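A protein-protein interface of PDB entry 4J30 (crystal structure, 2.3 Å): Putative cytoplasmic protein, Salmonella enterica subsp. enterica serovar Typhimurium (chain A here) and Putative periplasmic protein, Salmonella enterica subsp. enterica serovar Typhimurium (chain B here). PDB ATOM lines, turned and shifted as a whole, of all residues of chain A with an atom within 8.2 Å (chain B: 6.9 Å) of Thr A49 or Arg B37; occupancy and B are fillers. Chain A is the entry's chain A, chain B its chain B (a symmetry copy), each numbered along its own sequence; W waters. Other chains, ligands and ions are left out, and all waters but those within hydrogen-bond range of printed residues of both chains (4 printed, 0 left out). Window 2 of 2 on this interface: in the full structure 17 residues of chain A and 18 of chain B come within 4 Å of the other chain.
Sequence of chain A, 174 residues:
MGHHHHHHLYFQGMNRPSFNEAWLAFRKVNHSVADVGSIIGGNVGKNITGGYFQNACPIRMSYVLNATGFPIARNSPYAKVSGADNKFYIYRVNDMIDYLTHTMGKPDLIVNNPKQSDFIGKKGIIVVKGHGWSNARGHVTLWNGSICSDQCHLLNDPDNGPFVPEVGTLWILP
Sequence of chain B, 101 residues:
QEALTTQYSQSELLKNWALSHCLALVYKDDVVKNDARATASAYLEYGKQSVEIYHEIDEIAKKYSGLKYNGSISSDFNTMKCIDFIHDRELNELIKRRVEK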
ATOM      1  N   VAL A  33     -20.738   5.855  -4.018  1.00  0.00           N
ATOM      2  CA  VAL A  33     -21.172   7.228  -3.825  1.00  0.00           C
ATOM      3  C   VAL A  33     -19.991   8.195  -3.588  1.00  0.00           C
ATOM      4  O   VAL A  33     -20.024   9.340  -4.053  1.00  0.00           O
ATOM      5  CB  VAL A  33     -22.282   7.327  -2.719  1.00  0.00           C
ATOM      6  CG1 VAL A  33     -21.727   6.956  -1.308  1.00  0.00           C
ATOM      7  CG2 VAL A  33     -22.944   8.695  -2.741  1.00  0.00           C
ATOM      8  N   ALA A  34     -18.947   7.724  -2.894  1.00  0.00           N
ATOM      9  CA  ALA A  34     -17.713   8.496  -2.721  1.00  0.00           C
ATOM     10  C   ALA A  34     -17.082   8.826  -4.071  1.00  0.00           C
ATOM     11  O   ALA A  34     -16.723   9.977  -4.325  1.00  0.00           O
ATOM     12  CB  ALA A  34     -16.706   7.757  -1.813  1.00  0.00           C
ATOM     13  N   GLY A  37     -18.958  11.418  -5.998  1.00  0.00           N
ATOM     14  CA  GLY A  37     -18.639  12.751  -5.482  1.00  0.00           C
ATOM     15  C   GLY A  37     -17.367  13.337  -6.067  1.00  0.00           C
ATOM     16  O   GLY A  37     -17.315  14.539  -6.329  1.00  0.00           O
ATOM     17  N   SER A  38     -16.351  12.485  -6.269  1.00  0.00           N
ATOM     18  CA  SER A  38     -15.072  12.870  -6.871  1.00  0.00           C
ATOM     19  C   SER A  38     -15.254  13.185  -8.338  1.00  0.00           C
ATOM     20  O   SER A  38     -14.633  14.114  -8.861  1.00  0.00           O
ATOM     21  CB  SER A  38     -14.041  11.740  -6.756  1.00  0.00           C
ATOM     22  OG  SER A  38     -13.698  11.485  -5.403  1.00  0.00           O
ATOM     23  N   GLY A  41     -17.939  16.539  -8.320  1.00  0.00           N
ATOM     24  CA  GLY A  41     -17.325  17.688  -7.672  1.00  0.00           C
ATOM     25  C   GLY A  41     -18.343  18.727  -7.244  1.00  0.00           C
ATOM     26  O   GLY A  41     -19.530  18.423  -7.126  1.00  0.00           O
ATOM     27  N   GLY A  42     -17.873  19.952  -6.994  1.00  0.00           N
ATOM     28  CA  GLY A  42     -18.730  21.049  -6.536  1.00  0.00           C
ATOM     29  C   GLY A  42     -19.490  20.655  -5.285  1.00  0.00           C
ATOM     30  O   GLY A  42     -18.972  19.892  -4.473  1.00  0.00           O
ATOM     31  N   ASN A  43     -20.714  21.165  -5.132  1.00  0.00           N
ATOM     32  CA  ASN A  43     -21.542  20.891  -3.950  1.00  0.00           C
ATOM     33  C   ASN A  43     -21.981  19.431  -3.808  1.00  0.00           C
ATOM     34  O   ASN A  43     -22.232  18.955  -2.698  1.00  0.00           O
ATOM     35  CB  ASN A  43     -22.753  21.834  -3.896  1.00  0.00           C
ATOM     36  CG  ASN A  43     -22.355  23.287  -3.624  1.00  0.00           C
ATOM     37  OD1 ASN A  43     -21.269  23.564  -3.113  1.00  0.00           O
ATOM     38  ND2 ASN A  43     -23.232  24.217  -3.978  1.00  0.00           N
ATOM     39  N   VAL A  44     -22.082  18.727  -4.929  1.00  0.00           N
ATOM     40  CA  VAL A  44     -22.327  17.278  -4.914  1.00  0.00           C
ATOM     41  C   VAL A  44     -21.174  16.602  -4.167  1.00  0.00           C
ATOM     42  O   VAL A  44     -21.400  15.867  -3.211  1.00  0.00           O
ATOM     43  CB  VAL A  44     -22.474  16.680  -6.351  1.00  0.00           C
ATOM     44  CG1 VAL A  44     -22.497  15.154  -6.311  1.00  0.00           C
ATOM     45  CG2 VAL A  44     -23.742  17.191  -7.019  1.00  0.00           C
ATOM     46  N   GLY A  45     -19.945  16.885  -4.605  1.00  0.00           N
ATOM     47  CA  GLY A  45     -18.751  16.341  -3.972  1.00  0.00           C
ATOM     48  C   GLY A  45     -18.596  16.718  -2.510  1.00  0.00           C
ATOM     49  O   GLY A  45     -18.259  15.870  -1.689  1.00  0.00           O
ATOM     50  N   LYS A  46     -18.831  17.992  -2.188  1.00  0.00           N
ATOM     51  CA  LYS A  46     -18.754  18.474  -0.805  1.00  0.00           C
ATOM     52  C   LYS A  46     -19.733  17.740   0.116  1.00  0.00           C
ATOM     53  O   LYS A  46     -19.374  17.353   1.228  1.00  0.00           O
ATOM     54  CB  LYS A  46     -18.994  19.992  -0.732  1.00  0.00           C
ATOM     55  CG  LYS A  46     -17.876  20.859  -1.366  1.00  0.00           C
ATOM     56  CD  LYS A  46     -18.119  22.352  -1.108  1.00  0.00           C
ATOM     57  CE  LYS A  46     -17.337  23.264  -2.085  1.00  0.00           C
ATOM     58  NZ  LYS A  46     -18.006  23.387  -3.458  1.00  0.00           N
ATOM     59  N   ASN A  47     -20.964  17.546  -0.352  1.00  0.00           N
ATOM     60  CA  ASN A  47     -21.987  16.851   0.437  1.00  0.00           C
ATOM     61  C   ASN A  47     -21.735  15.360   0.596  1.00  0.00           C
ATOM     62  O   ASN A  47     -22.001  14.802   1.648  1.00  0.00           O
ATOM     63  CB  ASN A  47     -23.387  17.108  -0.126  1.00  0.00           C
ATOM     64  CG  ASN A  47     -23.942  18.446   0.306  1.00  0.00           C
ATOM     65  OD1 ASN A  47     -24.412  18.595   1.435  1.00  0.00           O
ATOM     66  ND2 ASN A  47     -23.890  19.434  -0.591  1.00  0.00           N
ATOM     67  N   ILE A  48     -21.209  14.718  -0.444  1.00  0.00           N
ATOM     68  CA  ILE A  48     -20.791  13.320  -0.341  1.00  0.00           C
ATOM     69  C   ILE A  48     -19.567  13.159   0.587  1.00  0.00           C
ATOM     70  O   ILE A  48     -19.546  12.262   1.426  1.00  0.00           O
ATOM     71  CB  ILE A  48     -20.560  12.695  -1.730  1.00  0.00           C
ATOM     72  CG1 ILE A  48     -21.916  12.512  -2.423  1.00  0.00           C
ATOM     73  CG2 ILE A  48     -19.785  11.369  -1.617  1.00  0.00           C
ATOM     74  CD1 ILE A  48     -21.834  12.234  -3.905  1.00  0.00           C
ATOM     75  N   THR A  49     -18.571  14.036   0.445  1.00  0.00           N
ATOM     76  CA  THR A  49     -17.420  14.066   1.366  1.00  0.00           C
ATOM     77  C   THR A  49     -17.877  14.230   2.829  1.00  0.00           C
ATOM     78  O   THR A  49     -17.367  13.536   3.724  1.00  0.00           O
ATOM     79  CB  THR A  49     -16.396  15.150   0.960  1.00  0.00           C
ATOM     80  OG1 THR A  49     -15.810  14.791  -0.294  1.00  0.00           O
ATOM     81  CG2 THR A  49     -15.266  15.292   1.982  1.00  0.00           C
ATOM     82  N   GLY A  50     -18.856  15.113   3.059  1.00  0.00           N
ATOM     83  CA  GLY A  50     -19.411  15.327   4.399  1.00  0.00           C
ATOM     84  C   GLY A  50     -20.308  14.182   4.856  1.00  0.00           C
ATOM     85  O   GLY A  50     -20.710  14.125   6.022  1.00  0.00           O
ATOM     86  N   GLY A  51     -20.630  13.268   3.942  1.00  0.00           N
ATOM     87  CA  GLY A  51     -21.474  12.114   4.267  1.00  0.00           C
ATOM     88  C   GLY A  51     -22.969  12.388   4.279  1.00  0.00           C
ATOM     89  O   GLY A  51     -23.747  11.552   4.738  1.00  0.00           O
ATOM     90  N   TYR A  52     -23.378  13.545   3.763  1.00  0.00           N
ATOM     91  CA  TYR A  52     -24.785  13.949   3.791  1.00  0.00           C
ATOM     92  C   TYR A  52     -25.577  13.143   2.778  1.00  0.00           C
ATOM     93  O   TYR A  52     -26.740  12.817   3.014  1.00  0.00           O
ATOM     94  CB  TYR A  52     -24.934  15.443   3.485  1.00  0.00           C
ATOM     95  CG  TYR A  52     -24.322  16.346   4.528  1.00  0.00           C
ATOM     96  CD1 TYR A  52     -25.066  16.764   5.612  1.00  0.00           C
ATOM     97  CD2 TYR A  52     -22.994  16.778   4.425  1.00  0.00           C
ATOM     98  CE1 TYR A  52     -24.524  17.588   6.594  1.00  0.00           C
ATOM     99  CE2 TYR A  52     -22.430  17.613   5.406  1.00  0.00           C
ATOM    100  CZ  TYR A  52     -23.222  18.007   6.484  1.00  0.00           C
ATOM    101  OH  TYR A  52     -22.737  18.832   7.460  1.00  0.00           O
ATOM    102  N   PHE A  53     -24.936  12.841   1.649  1.00  0.00           N
ATOM    103  CA  PHE A  53     -25.523  12.001   0.614  1.00  0.00           C
ATOM    104  C   PHE A  53     -24.824  10.645   0.631  1.00  0.00           C
ATOM    105  O   PHE A  53     -23.593  10.568   0.588  1.00  0.00           O
ATOM    106  CB  PHE A  53     -25.389  12.627  -0.794  1.00  0.00           C
ATOM    107  CG  PHE A  53     -25.943  14.043  -0.931  1.00  0.00           C
ATOM    108  CD1 PHE A  53     -26.908  14.542  -0.053  1.00  0.00           C
ATOM    109  CD2 PHE A  53     -25.533  14.846  -1.998  1.00  0.00           C
ATOM    110  CE1 PHE A  53     -27.417  15.841  -0.200  1.00  0.00           C
ATOM    111  CE2 PHE A  53     -26.038  16.144  -2.168  1.00  0.00           C
ATOM    112  CZ  PHE A  53     -26.976  16.646  -1.272  1.00  0.00           C
ATOM    113  N   GLN A  54     -25.627   9.588   0.698  1.00  0.00           N
ATOM    114  CA  GLN A  54     -25.159   8.206   0.687  1.00  0.00           C
ATOM    115  C   GLN A  54     -25.841   7.384  -0.419  1.00  0.00           C
ATOM    116  O   GLN A  54     -25.312   6.361  -0.851  1.00  0.00           O
ATOM    117  CB  GLN A  54     -25.398   7.543   2.066  1.00  0.00           C
ATOM    118  CG  GLN A  54     -24.546   8.112   3.198  1.00  0.00           C
ATOM    119  CD  GLN A  54     -23.064   7.814   3.018  1.00  0.00           C
ATOM    120  OE1 GLN A  54     -22.598   6.724   3.325  1.00  0.00           O
ATOM    121  NE2 GLN A  54     -22.321   8.788   2.513  1.00  0.00           N
ATOM    122  N   ASN A  55     -27.026   7.817  -0.845  1.00  0.00           N
ATOM    123  CA  ASN A  55     -27.738   7.183  -1.971  1.00  0.00           C
ATOM    124  C   ASN A  55     -27.451   7.921  -3.276  1.00  0.00           C
ATOM    125  O   ASN A  55     -27.963   9.033  -3.506  1.00  0.00           O
ATOM    126  CB  ASN A  55     -29.250   7.099  -1.708  1.00  0.00           C
ATOM    127  CG  ASN A  55     -29.981   6.169  -2.685  1.00  0.00           C
ATOM    128  OD1 ASN A  55     -29.385   5.595  -3.607  1.00  0.00           O
ATOM    129  ND2 ASN A  55     -31.286   6.004  -2.464  1.00  0.00           N
ATOM    130  N   TRP B  17     -32.432  12.509  12.165  1.00  0.00           N
ATOM    131  CA  TRP B  17     -31.235  12.831  11.392  1.00  0.00           C
ATOM    132  C   TRP B  17     -30.124  13.371  12.298  1.00  0.00           C
ATOM    133  O   TRP B  17     -28.966  12.930  12.221  1.00  0.00           O
ATOM    134  CB  TRP B  17     -31.541  13.853  10.292  1.00  0.00           C
ATOM    135  CG  TRP B  17     -30.399  13.951   9.311  1.00  0.00           C
ATOM    136  CD1 TRP B  17     -30.256  13.243   8.161  1.00  0.00           C
ATOM    137  CD2 TRP B  17     -29.223  14.770   9.433  1.00  0.00           C
ATOM    138  NE1 TRP B  17     -29.072  13.580   7.540  1.00  0.00           N
ATOM    139  CE2 TRP B  17     -28.414  14.506   8.306  1.00  0.00           C
ATOM    140  CE3 TRP B  17     -28.780  15.714  10.380  1.00  0.00           C
ATOM    141  CZ2 TRP B  17     -27.179  15.154   8.096  1.00  0.00           C
ATOM    142  CZ3 TRP B  17     -27.562  16.345  10.173  1.00  0.00           C
ATOM    143  CH2 TRP B  17     -26.779  16.068   9.038  1.00  0.00           C
ATOM    144  N   SER B  20     -28.543  10.468  14.509  1.00  0.00           N
ATOM    145  CA  SER B  20     -27.742   9.512  13.754  1.00  0.00           C
ATOM    146  C   SER B  20     -26.493  10.138  13.156  1.00  0.00           C
ATOM    147  O   SER B  20     -25.419   9.513  13.133  1.00  0.00           O
ATOM    148  CB  SER B  20     -28.574   8.800  12.684  1.00  0.00           C
ATOM    149  OG  SER B  20     -29.386   9.707  11.989  1.00  0.00           O
ATOM    150  N   HIS B  21     -26.630  11.372  12.677  1.00  0.00           N
ATOM    151  CA  HIS B  21     -25.496  12.097  12.124  1.00  0.00           C
ATOM    152  C   HIS B  21     -24.453  12.370  13.213  1.00  0.00           C
ATOM    153  O   HIS B  21     -23.248  12.222  12.975  1.00  0.00           O
ATOM    154  CB  HIS B  21     -25.948  13.416  11.499  1.00  0.00           C
ATOM    155  CG  HIS B  21     -24.814  14.320  11.131  1.00  0.00           C
ATOM    156  ND1 HIS B  21     -24.029  14.112  10.020  1.00  0.00           N
ATOM    157  CD2 HIS B  21     -24.326  15.429  11.733  1.00  0.00           C
ATOM    158  CE1 HIS B  21     -23.108  15.053   9.950  1.00  0.00           C
ATOM    159  NE2 HIS B  21     -23.264  15.863  10.980  1.00  0.00           N
ATOM    160  N   LEU B  23     -23.969  10.583  15.840  1.00  0.00           N
ATOM    161  CA  LEU B  23     -23.311   9.294  16.105  1.00  0.00           C
ATOM    162  C   LEU B  23     -22.259   8.969  15.039  1.00  0.00           C
ATOM    163  O   LEU B  23     -21.198   8.421  15.345  1.00  0.00           O
ATOM    164  CB  LEU B  23     -24.331   8.165  16.262  1.00  0.00           C
ATOM    165  CG  LEU B  23     -25.282   8.281  17.464  1.00  0.00           C
ATOM    166  CD1 LEU B  23     -26.458   7.299  17.315  1.00  0.00           C
ATOM    167  CD2 LEU B  23     -24.553   8.074  18.827  1.00  0.00           C
ATOM    168  N   ALA B  24     -22.555   9.327  13.793  1.00  0.00           N
ATOM    169  CA  ALA B  24     -21.584   9.227  12.700  1.00  0.00           C
ATOM    170  C   ALA B  24     -20.335  10.076  12.934  1.00  0.00           C
ATOM    171  O   ALA B  24     -19.242   9.690  12.528  1.00  0.00           O
ATOM    172  CB  ALA B  24     -22.242   9.588  11.360  1.00  0.00           C
ATOM    173  N   LEU B  25     -20.489  11.223  13.590  1.00  0.00           N
ATOM    174  CA  LEU B  25     -19.327  12.073  13.939  1.00  0.00           C
ATOM    175  C   LEU B  25     -18.431  11.523  15.060  1.00  0.00           C
ATOM    176  O   LEU B  25     -17.204  11.583  14.956  1.00  0.00           O
ATOM    177  CB  LEU B  25     -19.766  13.493  14.316  1.00  0.00           C
ATOM    178  CG  LEU B  25     -20.459  14.377  13.279  1.00  0.00           C
ATOM    179  CD1 LEU B  25     -20.967  15.654  13.953  1.00  0.00           C
ATOM    180  CD2 LEU B  25     -19.520  14.717  12.124  1.00  0.00           C
ATOM    181  N   VAL B  32     -19.426   1.198  12.044  1.00  0.00           N
ATOM    182  CA  VAL B  32     -20.350   2.018  12.833  1.00  0.00           C
ATOM    183  C   VAL B  32     -20.631   3.398  12.203  1.00  0.00           C
ATOM    184  O   VAL B  32     -21.796   3.791  12.093  1.00  0.00           O
ATOM    185  CB  VAL B  32     -19.875   2.182  14.315  1.00  0.00           C
ATOM    186  CG1 VAL B  32     -20.782   3.105  15.065  1.00  0.00           C
ATOM    187  CG2 VAL B  32     -19.850   0.848  15.021  1.00  0.00           C
ATOM    188  N   LYS B  33     -19.571   4.125  11.819  1.00  0.00           N
ATOM    189  CA  LYS B  33     -19.703   5.416  11.115  1.00  0.00           C
ATOM    190  C   LYS B  33     -20.534   5.282   9.841  1.00  0.00           C
ATOM    191  O   LYS B  33     -21.455   6.062   9.626  1.00  0.00           O
ATOM    192  CB  LYS B  33     -18.337   6.016  10.738  1.00  0.00           C
ATOM    193  CG  LYS B  33     -17.465   6.453  11.910  1.00  0.00           C
ATOM    194  CD  LYS B  33     -16.132   7.074  11.416  1.00  0.00           C
ATOM    195  CE  LYS B  33     -16.187   8.600  11.386  1.00  0.00           C
ATOM    196  NZ  LYS B  33     -16.562   9.167  12.729  1.00  0.00           N
ATOM    197  N   ASN B  34     -20.212   4.303   8.999  1.00  0.00           N
ATOM    198  CA  ASN B  34     -20.989   4.076   7.778  1.00  0.00           C
ATOM    199  C   ASN B  34     -22.455   3.784   8.058  1.00  0.00           C
ATOM    200  O   ASN B  34     -23.337   4.308   7.383  1.00  0.00           O
ATOM    201  CB  ASN B  34     -20.383   2.955   6.930  1.00  0.00           C
ATOM    202  CG  ASN B  34     -19.051   3.342   6.329  1.00  0.00           C
ATOM    203  OD1 ASN B  34     -18.804   4.523   6.050  1.00  0.00           O
ATOM    204  ND2 ASN B  34     -18.183   2.358   6.135  1.00  0.00           N
ATOM    205  N   ASP B  35     -22.693   2.960   9.071  1.00  0.00           N
ATOM    206  CA  ASP B  35     -24.034   2.584   9.485  1.00  0.00           C
ATOM    207  C   ASP B  35     -24.842   3.816   9.876  1.00  0.00           C
ATOM    208  O   ASP B  35     -25.951   4.013   9.372  1.00  0.00           O
ATOM    209  CB  ASP B  35     -23.950   1.593  10.643  1.00  0.00           C
ATOM    210  CG  ASP B  35     -25.281   0.980  10.979  1.00  0.00           C
ATOM    211  OD1 ASP B  35     -25.525  -0.159  10.539  1.00  0.00           O
ATOM    212  OD2 ASP B  35     -26.084   1.636  11.675  1.00  0.00           O
ATOM    213  N   ALA B  36     -24.275   4.642  10.761  1.00  0.00           N
ATOM    214  CA  ALA B  36     -24.908   5.886  11.193  1.00  0.00           C
ATOM    215  C   ALA B  36     -25.101   6.880  10.053  1.00  0.00           C
ATOM    216  O   ALA B  36     -26.140   7.543   9.988  1.00  0.00           O
ATOM    217  CB  ALA B  36     -24.116   6.528  12.318  1.00  0.00           C
ATOM    218  N   ARG B  37     -24.099   6.987   9.174  1.00  0.00           N
ATOM    219  CA  ARG B  37     -24.219   7.750   7.931  1.00  0.00           C
ATOM    220  C   ARG B  37     -25.369   7.274   7.045  1.00  0.00           C
ATOM    221  O   ARG B  37     -26.111   8.087   6.498  1.00  0.00           O
ATOM    222  CB  ARG B  37     -22.937   7.659   7.105  1.00  0.00           C
ATOM    223  CG  ARG B  37     -21.867   8.623   7.472  1.00  0.00           C
ATOM    224  CD  ARG B  37     -20.770   8.598   6.422  1.00  0.00           C
ATOM    225  NE  ARG B  37     -19.653   9.462   6.782  1.00  0.00           N
ATOM    226  CZ  ARG B  37     -18.766   9.960   5.920  1.00  0.00           C
ATOM    227  NH1 ARG B  37     -18.842   9.672   4.623  1.00  0.00           N
ATOM    228  NH2 ARG B  37     -17.791  10.751   6.358  1.00  0.00           N
ATOM    229  N   ALA B  38     -25.485   5.962   6.878  1.00  0.00           N
ATOM    230  CA  ALA B  38     -26.517   5.374   6.020  1.00  0.00           C
ATOM    231  C   ALA B  38     -27.905   5.634   6.616  1.00  0.00           C
ATOM    232  O   ALA B  38     -28.850   5.976   5.890  1.00  0.00           O
ATOM    233  CB  ALA B  38     -26.279   3.893   5.843  1.00  0.00           C
ATOM    234  N   THR B  39     -28.002   5.477   7.937  1.00  0.00           N
ATOM    235  CA  THR B  39     -29.217   5.727   8.692  1.00  0.00           C
ATOM    236  C   THR B  39     -29.672   7.195   8.590  1.00  0.00           C
ATOM    237  O   THR B  39     -30.852   7.460   8.338  1.00  0.00           O
ATOM    238  CB  THR B  39     -29.031   5.318  10.176  1.00  0.00           C
ATOM    239  OG1 THR B  39     -28.761   3.909  10.255  1.00  0.00           O
ATOM    240  CG2 THR B  39     -30.263   5.660  11.006  1.00  0.00           C
ATOM    241  N   ALA B  40     -28.750   8.135   8.805  1.00  0.00           N
ATOM    242  CA  ALA B  40     -29.042   9.552   8.610  1.00  0.00           C
ATOM    243  C   ALA B  40     -29.587   9.852   7.195  1.00  0.00           C
ATOM    244  O   ALA B  40     -30.577  10.578   7.059  1.00  0.00           O
ATOM    245  CB  ALA B  40     -27.783  10.429   8.911  1.00  0.00           C
ATOM    246  N   SER B  41     -28.970   9.270   6.157  1.00  0.00           N
ATOM    247  CA  SER B  41     -29.409   9.522   4.772  1.00  0.00           C
ATOM    248  C   SER B  41     -30.864   9.110   4.529  1.00  0.00           C
ATOM    249  O   SER B  41     -31.581   9.758   3.743  1.00  0.00           O
ATOM    250  CB  SER B  41     -28.461   8.870   3.749  1.00  0.00           C
ATOM    251  OG  SER B  41     -28.714   7.484   3.592  1.00  0.00           O
ATOM    252  N   ALA B  42     -31.303   8.041   5.198  1.00  0.00           N
ATOM    253  CA  ALA B  42     -32.697   7.627   5.135  1.00  0.00           C
ATOM    254  C   ALA B  42     -33.663   8.735   5.608  1.00  0.00           C
ATOM    255  O   ALA B  42     -34.692   8.961   4.985  1.00  0.00           O
ATOM    256  CB  ALA B  42     -32.911   6.359   5.948  1.00  0.00           C
HETATM  257  O   HOH W   1     -25.676  10.762   6.299  1.00  0.00           O
HETATM  258  O   HOH W   2     -27.758  12.262   5.472  1.00  0.00           O
HETATM  259  O   HOH W   3     -19.748   6.487   4.003  1.00  0.00           O
HETATM  260  O   HOH W   4     -22.989   4.593   4.686  1.00  0.00           O
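Ala A34 touches none of the printed residues of chain B.
Thr A49 touches just one residue of chain B: Arg B37.
Of the printed residues of chain B, Gly A51 touches Arg B37.
Of the printed residues of chain B, Tyr A52 touches Trp B17.
Of the printed residues of chain B, Gln A54 touches Arg B37 and Ser B41.
Of the printed residues of chain A, Trp B17 touches Tyr A52 (3.6 Å).
Ser B20 touches none of the printed residues of chain A.
Ala B36 touches none of the printed residues of chain A.
Of chain A, only Thr A49, Gly A51 and Gln A54 come within 4 Å of Arg B37.
The nearest residue of chain A that does not touch Arg B37 is Ile A48 (4.2 Å).
The nearest printed residue of chain B that does not touch Tyr A52 is Ser B41 (4.4 Å).
Among the printed residues, merely in contact across the chains: Gly A51 with Arg B37 (3.6 Å), Tyr A52 with Trp B17 (3.6 Å), Gln A54 with Ser B41 (3.7 Å), Gln A54 with Arg B37 (3.7 Å) and Thr A49 with Arg B37 (3.9 Å).
O of Ala B38 is in hydrogen-bond range of OG of Ser B41, at 2.8 Å.
The backbone carbonyl oxygen (O) of Trp B17 sits at hydrogen-bond distance from the side-chain hydroxyl (OG) of Ser B20, 3.3 Å away.
The indole nitrogen (NE1) of Trp B17 sits close to the backbone carbonyl oxygen (O) of Ala B40 (3.4 Å).
The backbone carbonyl oxygen of Asn A47 lies within hydrogen-bond range of the backbone NH of Tyr A52 (2.8 Å).
OG1 of Thr A49 lies within hydrogen-bond range of O of Gly A45.
Hydrophobic or aromatic side chains of chain A within 4 Å of the printed part of chain B: Tyr A52.
Of the 17 printed residues of chain B, 3 touch a printed residue of chain A.
Among the printed residues, 5 pairs touch across the chains.
Among the printed residues, no Asp or Glu carboxylate lies within 4 Å of a Lys or Arg side-chain nitrogen of the other chain.
Water W4 bridges the side-chain amide oxygen (OE1) of Gln A54 and the backbone carbonyl oxygen (O) of Asn B34.
Water W1 lies within hydrogen-bond range of O of Gly A51 (2.6 Å) and O of Arg B37 (2.7 Å).
Water W2 lies within hydrogen-bond range of the backbone carbonyl oxygen of Tyr A52 (2.7 Å), the indole nitrogen of Trp B17 (2.8 Å) and the backbone NH of Ser B41 (3.3 Å).
Water W3 lies within hydrogen-bond range of the side-chain amide oxygen (OE1) of Gln A54, the side-chain amide oxygen (OD1) of Asn B34 and the guanidinium group (NH1) of Arg B37.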
